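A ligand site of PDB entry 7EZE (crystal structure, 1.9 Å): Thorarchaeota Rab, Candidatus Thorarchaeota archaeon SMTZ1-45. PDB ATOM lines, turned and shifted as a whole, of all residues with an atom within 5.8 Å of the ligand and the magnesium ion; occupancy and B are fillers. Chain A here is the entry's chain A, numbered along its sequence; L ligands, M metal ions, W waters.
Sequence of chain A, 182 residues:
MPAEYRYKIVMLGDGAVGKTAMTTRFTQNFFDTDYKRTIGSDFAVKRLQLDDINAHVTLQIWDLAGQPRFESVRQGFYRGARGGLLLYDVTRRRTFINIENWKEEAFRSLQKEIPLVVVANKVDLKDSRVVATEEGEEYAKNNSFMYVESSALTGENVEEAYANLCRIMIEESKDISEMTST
An oxygen (O7) of the ligand sits at hydrogen-bond distance from the backbone NH (N) of Thr 20, at 3.5 Å.
An oxygen (O4) of the ligand is in hydrogen-bond range of the backbone NH (N) of Lys 19, at 3.0 Å.
NZ of Lys 19 lies within salt-bridge range of O4 of the ligand (2.7 Å).
OD1 of Asp 124 is in hydrogen-bond range of N3 of the ligand (2.7 Å).
An oxygen (O7) of the ligand is in hydrogen-bond range of the backbone NH of Ala 21, 2.8 Å away.
An oxygen (O13) of the ligand is in hydrogen-bond range of the backbone NH (N) of Ala 152.
N of Gly 18 lies within hydrogen-bond range of O8 of the ligand, 2.9 Å away.
N of Ala 16 sits at hydrogen-bond distance from O1 of the ligand, 2.9 Å away.
The side-chain amide nitrogen (ND2) of Asn 121 lies within hydrogen-bond range of a nitrogen (N2) of the ligand.
The backbone NH of Val 17 is in hydrogen-bond range of an oxygen (O4) of the ligand.
NZ of Lys 122 is in hydrogen-bond range of O10 of the ligand (3.4 Å).
O13 of the ligand sits at hydrogen-bond distance from N of Leu 153 (3.5 Å).
OG1 of Thr 20 sits close to OD2 of Asp 63 (2.8 Å).
The backbone carbonyl oxygen (O) of Asp 14 sits at hydrogen-bond distance from the side-chain amino group (NZ) of Lys 19, at 2.8 Å.
O of Gly 13 sits at hydrogen-bond distance from NZ of Lys 19.
OD1 of Asp 124 is in hydrogen-bond range of OG of Ser 151 (2.7 Å).
The backbone carbonyl oxygen (O) of Ala 16 sits at hydrogen-bond distance from the side-chain amino group (NZ) of Lys 122 (2.8 Å).
O of Val 17 sits at hydrogen-bond distance from ND2 of Asn 121 (2.8 Å).
The side-chain amide oxygen (OD1) of Asn 121 lies within hydrogen-bond range of the side-chain hydroxyl (OG) of Ser 150 (2.9 Å).
The backbone carbonyl oxygen (O) of Ser 150 sits at hydrogen-bond distance from the backbone NH (N) of Lys 122 (3.1 Å).
Residues that only touch the ligand: Asp 14 (3.9 Å), Gly 15 (3.7 Å), Phe 31 (3.3 Å), Thr 33 (3.96 Å), Leu 125 (3.5 Å) and Ser 151 (3.4 Å).
Hydrophobic or aromatic side chains within 4 Å of the ligand: Ala 16, Val 17, Ala 21, Phe 31, Leu 125, Ala 152 and Leu 153.
Of the 24 residues printed, 17 come within 4 Å of the ligand.
The nearest printed residue that does not touch the ligand is Asp 32 (4.6 Å).
The magnesium ion is bound by an oxygen (O5) of the ligand (2.0 Å), water W4 (2.1 Å), the side-chain hydroxyl (OG1) of Thr 20 (2.2 Å), water W2 (2.2 Å), an oxygen (O3) of the ligand (2.3 Å) and water W6 (2.3 Å).
The magnesium ion has six donor atoms within binding distance.
Water W4 bridges OD1 of Asp 63 (2.7 Å) and O2 of the ligand (3.0 Å).
Water W8 lies within hydrogen-bond range of an oxygen (O12) of the ligand and the backbone carbonyl oxygen of Asp 32.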
ATOM      1  N   GLY A  13     -12.386   9.609 -13.840  1.00  0.00           N
ATOM      2  CA  GLY A  13     -11.435   8.527 -13.597  1.00  0.00           C
ATOM      3  C   GLY A  13     -12.131   7.220 -13.271  1.00  0.00           C
ATOM      4  O   GLY A  13     -13.299   7.175 -12.904  1.00  0.00           O
ATOM      5  N   ASP A  14     -11.365   6.131 -13.388  1.00  0.00           N
ATOM      6  CA  ASP A  14     -11.876   4.782 -13.166  1.00  0.00           C
ATOM      7  C   ASP A  14     -12.342   4.605 -11.715  1.00  0.00           C
ATOM      8  O   ASP A  14     -12.155   5.457 -10.852  1.00  0.00           O
ATOM      9  CB  ASP A  14     -10.803   3.738 -13.474  1.00  0.00           C
ATOM     10  CG  ASP A  14     -10.610   3.524 -14.955  1.00  0.00           C
ATOM     11  OD1 ASP A  14     -11.298   4.178 -15.757  1.00  0.00           O
ATOM     12  OD2 ASP A  14      -9.750   2.688 -15.322  1.00  0.00           O
ATOM     13  N   GLY A  15     -12.947   3.440 -11.462  1.00  0.00           N
ATOM     14  CA  GLY A  15     -13.405   3.144 -10.125  1.00  0.00           C
ATOM     15  C   GLY A  15     -12.240   3.033  -9.141  1.00  0.00           C
ATOM     16  O   GLY A  15     -11.180   2.513  -9.472  1.00  0.00           O
ATOM     17  N   ALA A  16     -12.464   3.553  -7.933  1.00  0.00           N
ATOM     18  CA  ALA A  16     -11.522   3.470  -6.814  1.00  0.00           C
ATOM     19  C   ALA A  16     -10.235   4.244  -7.046  1.00  0.00           C
ATOM     20  O   ALA A  16      -9.227   3.967  -6.372  1.00  0.00           O
ATOM     21  CB  ALA A  16     -11.206   2.016  -6.459  1.00  0.00           C
ATOM     22  N   VAL A  17     -10.201   5.214  -7.959  1.00  0.00           N
ATOM     23  CA  VAL A  17      -9.004   6.046  -8.103  1.00  0.00           C
ATOM     24  C   VAL A  17      -8.921   7.120  -7.029  1.00  0.00           C
ATOM     25  O   VAL A  17      -7.846   7.692  -6.819  1.00  0.00           O
ATOM     26  CB  VAL A  17      -8.904   6.714  -9.487  1.00  0.00           C
ATOM     27  CG1 VAL A  17      -8.806   5.666 -10.589  1.00  0.00           C
ATOM     28  CG2 VAL A  17     -10.077   7.662  -9.715  1.00  0.00           C
ATOM     29  N   GLY A  18     -10.018   7.404  -6.349  1.00  0.00           N
ATOM     30  CA  GLY A  18     -10.042   8.413  -5.304  1.00  0.00           C
ATOM     31  C   GLY A  18     -10.836   9.674  -5.623  1.00  0.00           C
ATOM     32  O   GLY A  18     -10.592  10.704  -4.981  1.00  0.00           O
ATOM     33  N   LYS A  19     -11.769   9.620  -6.570  1.00  0.00           N
ATOM     34  CA  LYS A  19     -12.554  10.812  -6.911  1.00  0.00           C
ATOM     35  C   LYS A  19     -13.302  11.342  -5.693  1.00  0.00           C
ATOM     36  O   LYS A  19     -13.229  12.530  -5.377  1.00  0.00           O
ATOM     37  CB  LYS A  19     -13.533  10.489  -8.045  1.00  0.00           C
ATOM     38  CG  LYS A  19     -12.861   9.977  -9.321  1.00  0.00           C
ATOM     39  CD  LYS A  19     -13.885   9.680 -10.426  1.00  0.00           C
ATOM     40  CE  LYS A  19     -14.804   8.521 -10.067  1.00  0.00           C
ATOM     41  NZ  LYS A  19     -14.070   7.235  -9.953  1.00  0.00           N
ATOM     42  N   THR A  20     -14.012  10.466  -4.984  1.00  0.00           N
ATOM     43  CA  THR A  20     -14.766  10.901  -3.818  1.00  0.00           C
ATOM     44  C   THR A  20     -13.841  11.355  -2.692  1.00  0.00           C
ATOM     45  O   THR A  20     -14.074  12.392  -2.068  1.00  0.00           O
ATOM     46  CB  THR A  20     -15.690   9.784  -3.337  1.00  0.00           C
ATOM     47  OG1 THR A  20     -16.542   9.370  -4.403  1.00  0.00           O
ATOM     48  CG2 THR A  20     -16.557  10.262  -2.160  1.00  0.00           C
ATOM     49  N   ALA A  21     -12.787  10.579  -2.421  1.00  0.00           N
ATOM     50  CA  ALA A  21     -11.874  10.938  -1.334  1.00  0.00           C
ATOM     51  C   ALA A  21     -11.197  12.268  -1.606  1.00  0.00           C
ATOM     52  O   ALA A  21     -10.980  13.055  -0.673  1.00  0.00           O
ATOM     53  CB  ALA A  21     -10.839   9.837  -1.135  1.00  0.00           C
ATOM     54  N   MET A  22     -10.875  12.548  -2.867  1.00  0.00           N
ATOM     55  CA  MET A  22     -10.277  13.837  -3.186  1.00  0.00           C
ATOM     56  C   MET A  22     -11.281  14.971  -2.969  1.00  0.00           C
ATOM     57  O   MET A  22     -10.925  16.024  -2.420  1.00  0.00           O
ATOM     58  CB  MET A  22      -9.766  13.832  -4.619  1.00  0.00           C
ATOM     59  CG  MET A  22      -8.987  15.075  -4.984  1.00  0.00           C
ATOM     60  SD  MET A  22      -8.052  14.852  -6.505  1.00  0.00           S
ATOM     61  CE  MET A  22      -7.073  16.356  -6.487  1.00  0.00           C
ATOM     62  N   PHE A  31     -10.165  12.740   5.842  1.00  0.00           N
ATOM     63  CA  PHE A  31     -10.048  11.491   5.111  1.00  0.00           C
ATOM     64  C   PHE A  31     -10.497  10.356   6.017  1.00  0.00           C
ATOM     65  O   PHE A  31     -10.163  10.337   7.200  1.00  0.00           O
ATOM     66  CB  PHE A  31      -8.601  11.254   4.630  1.00  0.00           C
ATOM     67  CG  PHE A  31      -8.380   9.931   3.937  1.00  0.00           C
ATOM     68  CD1 PHE A  31      -7.961   8.821   4.655  1.00  0.00           C
ATOM     69  CD2 PHE A  31      -8.563   9.816   2.572  1.00  0.00           C
ATOM     70  CE1 PHE A  31      -7.751   7.605   4.015  1.00  0.00           C
ATOM     71  CE2 PHE A  31      -8.358   8.610   1.930  1.00  0.00           C
ATOM     72  CZ  PHE A  31      -7.947   7.495   2.654  1.00  0.00           C
ATOM     73  N   ASP A  32     -11.267   9.418   5.457  1.00  0.00           N
ATOM     74  CA  ASP A  32     -11.793   8.297   6.227  1.00  0.00           C
ATOM     75  C   ASP A  32     -12.007   7.134   5.266  1.00  0.00           C
ATOM     76  O   ASP A  32     -12.742   7.265   4.282  1.00  0.00           O
ATOM     77  CB  ASP A  32     -13.106   8.680   6.911  1.00  0.00           C
ATOM     78  CG  ASP A  32     -13.546   7.670   7.969  1.00  0.00           C
ATOM     79  OD1 ASP A  32     -13.095   6.500   7.924  1.00  0.00           O
ATOM     80  OD2 ASP A  32     -14.351   8.049   8.848  1.00  0.00           O
ATOM     81  N   THR A  33     -11.351   5.998   5.552  1.00  0.00           N
ATOM     82  CA  THR A  33     -11.524   4.812   4.720  1.00  0.00           C
ATOM     83  C   THR A  33     -12.974   4.361   4.674  1.00  0.00           C
ATOM     84  O   THR A  33     -13.432   3.786   3.678  1.00  0.00           O
ATOM     85  CB  THR A  33     -10.639   3.675   5.253  1.00  0.00           C
ATOM     86  OG1 THR A  33      -9.295   4.127   5.380  1.00  0.00           O
ATOM     87  CG2 THR A  33     -10.679   2.474   4.312  1.00  0.00           C
ATOM     88  N   ASP A  63     -19.533  14.422  -8.946  1.00  0.00           N
ATOM     89  CA  ASP A  63     -18.786  13.184  -8.743  1.00  0.00           C
ATOM     90  C   ASP A  63     -19.786  12.026  -8.771  1.00  0.00           C
ATOM     91  O   ASP A  63     -20.429  11.741  -7.756  1.00  0.00           O
ATOM     92  CB  ASP A  63     -18.012  13.226  -7.433  1.00  0.00           C
ATOM     93  CG  ASP A  63     -17.438  11.888  -7.042  1.00  0.00           C
ATOM     94  OD1 ASP A  63     -16.806  11.232  -7.893  1.00  0.00           O
ATOM     95  OD2 ASP A  63     -17.603  11.496  -5.862  1.00  0.00           O
ATOM     96  N   ASN A 121      -3.113  10.231  -8.391  1.00  0.00           N
ATOM     97  CA  ASN A 121      -3.545  10.143  -7.006  1.00  0.00           C
ATOM     98  C   ASN A 121      -2.960   8.912  -6.312  1.00  0.00           C
ATOM     99  O   ASN A 121      -2.492   7.959  -6.948  1.00  0.00           O
ATOM    100  CB  ASN A 121      -5.075  10.102  -6.909  1.00  0.00           C
ATOM    101  CG  ASN A 121      -5.587  10.346  -5.497  1.00  0.00           C
ATOM    102  OD1 ASN A 121      -5.064  11.187  -4.770  1.00  0.00           O
ATOM    103  ND2 ASN A 121      -6.597   9.583  -5.097  1.00  0.00           N
ATOM    104  N   LYS A 122      -3.011   8.950  -4.972  1.00  0.00           N
ATOM    105  CA  LYS A 122      -2.525   7.897  -4.073  1.00  0.00           C
ATOM    106  C   LYS A 122      -1.000   7.789  -4.080  1.00  0.00           C
ATOM    107  O   LYS A 122      -0.447   6.704  -3.900  1.00  0.00           O
ATOM    108  CB  LYS A 122      -3.125   6.524  -4.418  1.00  0.00           C
ATOM    109  CG  LYS A 122      -4.647   6.472  -4.409  1.00  0.00           C
ATOM    110  CD  LYS A 122      -5.102   5.012  -4.390  1.00  0.00           C
ATOM    111  CE  LYS A 122      -6.591   4.873  -4.651  1.00  0.00           C
ATOM    112  NZ  LYS A 122      -6.981   3.429  -4.751  1.00  0.00           N
ATOM    113  N   VAL A 123      -0.302   8.915  -4.261  1.00  0.00           N
ATOM    114  CA  VAL A 123       1.154   8.875  -4.314  1.00  0.00           C
ATOM    115  C   VAL A 123       1.786   8.567  -2.959  1.00  0.00           C
ATOM    116  O   VAL A 123       2.996   8.316  -2.903  1.00  0.00           O
ATOM    117  CB  VAL A 123       1.705  10.211  -4.870  1.00  0.00           C
ATOM    118  CG1 VAL A 123       1.138  10.468  -6.262  1.00  0.00           C
ATOM    119  CG2 VAL A 123       1.387  11.361  -3.932  1.00  0.00           C
ATOM    120  N   ASP A 124       1.002   8.575  -1.881  1.00  0.00           N
ATOM    121  CA  ASP A 124       1.524   8.147  -0.589  1.00  0.00           C
ATOM    122  C   ASP A 124       1.860   6.669  -0.568  1.00  0.00           C
ATOM    123  O   ASP A 124       2.668   6.238   0.266  1.00  0.00           O
ATOM    124  CB  ASP A 124       0.531   8.486   0.528  1.00  0.00           C
ATOM    125  CG  ASP A 124      -0.832   7.859   0.326  1.00  0.00           C
ATOM    126  OD1 ASP A 124      -1.594   8.318  -0.557  1.00  0.00           O
ATOM    127  OD2 ASP A 124      -1.162   6.884   1.041  1.00  0.00           O
ATOM    128  N   LEU A 125       1.271   5.875  -1.470  1.00  0.00           N
ATOM    129  CA  LEU A 125       1.501   4.434  -1.550  1.00  0.00           C
ATOM    130  C   LEU A 125       2.761   4.158  -2.379  1.00  0.00           C
ATOM    131  O   LEU A 125       2.718   3.578  -3.472  1.00  0.00           O
ATOM    132  CB  LEU A 125       0.278   3.736  -2.133  1.00  0.00           C
ATOM    133  CG  LEU A 125      -1.029   3.887  -1.342  1.00  0.00           C
ATOM    134  CD1 LEU A 125      -2.188   3.252  -2.094  1.00  0.00           C
ATOM    135  CD2 LEU A 125      -0.892   3.273   0.053  1.00  0.00           C
ATOM    136  N   SER A 150      -1.059  13.855  -6.193  1.00  0.00           N
ATOM    137  CA  SER A 150      -1.910  14.162  -5.047  1.00  0.00           C
ATOM    138  C   SER A 150      -2.087  12.945  -4.160  1.00  0.00           C
ATOM    139  O   SER A 150      -1.856  11.795  -4.562  1.00  0.00           O
ATOM    140  CB  SER A 150      -3.286  14.667  -5.498  1.00  0.00           C
ATOM    141  OG  SER A 150      -4.060  13.597  -5.997  1.00  0.00           O
ATOM    142  N   SER A 151      -2.510  13.218  -2.925  1.00  0.00           N
ATOM    143  CA  SER A 151      -2.906  12.180  -1.972  1.00  0.00           C
ATOM    144  C   SER A 151      -4.097  12.708  -1.183  1.00  0.00           C
ATOM    145  O   SER A 151      -3.962  13.663  -0.420  1.00  0.00           O
ATOM    146  CB  SER A 151      -1.766  11.803  -1.037  1.00  0.00           C
ATOM    147  OG  SER A 151      -2.203  10.873  -0.066  1.00  0.00           O
ATOM    148  N   ALA A 152      -5.269  12.106  -1.393  1.00  0.00           N
ATOM    149  CA  ALA A 152      -6.419  12.432  -0.566  1.00  0.00           C
ATOM    150  C   ALA A 152      -6.150  12.101   0.891  1.00  0.00           C
ATOM    151  O   ALA A 152      -6.645  12.785   1.795  1.00  0.00           O
ATOM    152  CB  ALA A 152      -7.656  11.693  -1.072  1.00  0.00           C
ATOM    153  N   LEU A 153      -5.352  11.052   1.152  1.00  0.00           N
ATOM    154  CA  LEU A 153      -5.065  10.646   2.529  1.00  0.00           C
ATOM    155  C   LEU A 153      -4.265  11.715   3.265  1.00  0.00           C
ATOM    156  O   LEU A 153      -4.647  12.138   4.363  1.00  0.00           O
ATOM    157  CB  LEU A 153      -4.329   9.307   2.527  1.00  0.00           C
ATOM    158  CG  LEU A 153      -4.124   8.581   3.861  1.00  0.00           C
ATOM    159  CD1 LEU A 153      -3.890   7.092   3.629  1.00  0.00           C
ATOM    160  CD2 LEU A 153      -2.954   9.159   4.653  1.00  0.00           C
ATOM    161  N   THR A 154      -3.135  12.144   2.702  1.00  0.00           N
ATOM    162  CA  THR A 154      -2.296  13.120   3.381  1.00  0.00           C
ATOM    163  C   THR A 154      -2.685  14.554   3.081  1.00  0.00           C
ATOM    164  O   THR A 154      -2.211  15.467   3.777  1.00  0.00           O
ATOM    165  CB  THR A 154      -0.823  12.916   3.002  1.00  0.00           C
ATOM    166  OG1 THR A 154      -0.623  13.269   1.621  1.00  0.00           O
ATOM    167  CG2 THR A 154      -0.409  11.456   3.213  1.00  0.00           C
HETATM  168  P1  LIG L   1     -15.795   4.984  -6.996  1.00  0.00           P
HETATM  169  O1  LIG L   1     -14.325   5.180  -6.368  1.00  0.00           O
HETATM  170  S1  LIG L   1     -15.959   3.372  -7.515  1.00  0.00           S
HETATM  171  O2  LIG L   1     -16.005   5.958  -8.163  1.00  0.00           O
HETATM  172  O3  LIG L   1     -16.847   5.284  -5.912  1.00  0.00           O
HETATM  173  P2  LIG L   1     -13.653   6.642  -6.205  1.00  0.00           P
HETATM  174  O4  LIG L   1     -13.048   7.092  -7.471  1.00  0.00           O
HETATM  175  O5  LIG L   1     -14.618   7.623  -5.675  1.00  0.00           O
HETATM  176  P3  LIG L   1     -12.657   6.421  -3.560  1.00  0.00           P
HETATM  177  O6  LIG L   1     -13.860   5.664  -3.174  1.00  0.00           O
HETATM  178  O7  LIG L   1     -12.719   7.826  -3.099  1.00  0.00           O
HETATM  179  O8  LIG L   1     -12.464   6.358  -5.165  1.00  0.00           O
HETATM  180  O9  LIG L   1     -11.314   5.683  -3.077  1.00  0.00           O
HETATM  181  C1  LIG L   1     -11.153   4.293  -3.242  1.00  0.00           C
HETATM  182  C2  LIG L   1     -10.341   3.727  -2.078  1.00  0.00           C
HETATM  183  O10 LIG L   1      -9.042   4.275  -2.117  1.00  0.00           O
HETATM  184  C3  LIG L   1     -10.920   4.118  -0.732  1.00  0.00           C
HETATM  185  O11 LIG L   1     -10.681   3.066   0.162  1.00  0.00           O
HETATM  186  C4  LIG L   1     -10.107   5.312  -0.304  1.00  0.00           C
HETATM  187  O12 LIG L   1     -10.029   5.411   1.103  1.00  0.00           O
HETATM  188  C5  LIG L   1      -8.760   4.993  -0.934  1.00  0.00           C
HETATM  189  N1  LIG L   1      -8.030   6.222  -1.288  1.00  0.00           N
HETATM  190  C6  LIG L   1      -8.528   7.291  -1.986  1.00  0.00           C
HETATM  191  N2  LIG L   1      -7.533   8.197  -2.120  1.00  0.00           N
HETATM  192  C7  LIG L   1      -6.412   7.713  -1.531  1.00  0.00           C
HETATM  193  C8  LIG L   1      -5.128   8.218  -1.380  1.00  0.00           C
HETATM  194  O13 LIG L   1      -4.826   9.326  -1.843  1.00  0.00           O
HETATM  195  N3  LIG L   1      -4.181   7.474  -0.724  1.00  0.00           N
HETATM  196  C9  LIG L   1      -4.503   6.237  -0.205  1.00  0.00           C
HETATM  197  N4  LIG L   1      -3.576   5.512   0.428  1.00  0.00           N
HETATM  198  N5  LIG L   1      -5.779   5.736  -0.361  1.00  0.00           N
HETATM  199  C10 LIG L   1      -6.717   6.462  -1.014  1.00  0.00           C
HETATM  200 MG    MG M   1     -16.612   7.491  -5.472  1.00  0.00          MG
HETATM  201  O   HOH W   1     -13.883   7.742  -0.305  1.00  0.00           O
HETATM  202  O   HOH W   2     -16.235   6.625  -3.516  1.00  0.00           O
HETATM  203  O   HOH W   3      -5.786   2.694  -0.153  1.00  0.00           O
HETATM  204  O   HOH W   4     -16.989   8.661  -7.227  1.00  0.00           O
HETATM  205  O   HOH W   5      -3.905   3.616   2.217  1.00  0.00           O
HETATM  206  O   HOH W   6     -18.881   7.684  -5.059  1.00  0.00           O
HETATM  207  O   HOH W   7     -17.850   3.592  -4.437  1.00  0.00           O
HETATM  208  O   HOH W   8     -11.875   7.414   1.421  1.00  0.00           O
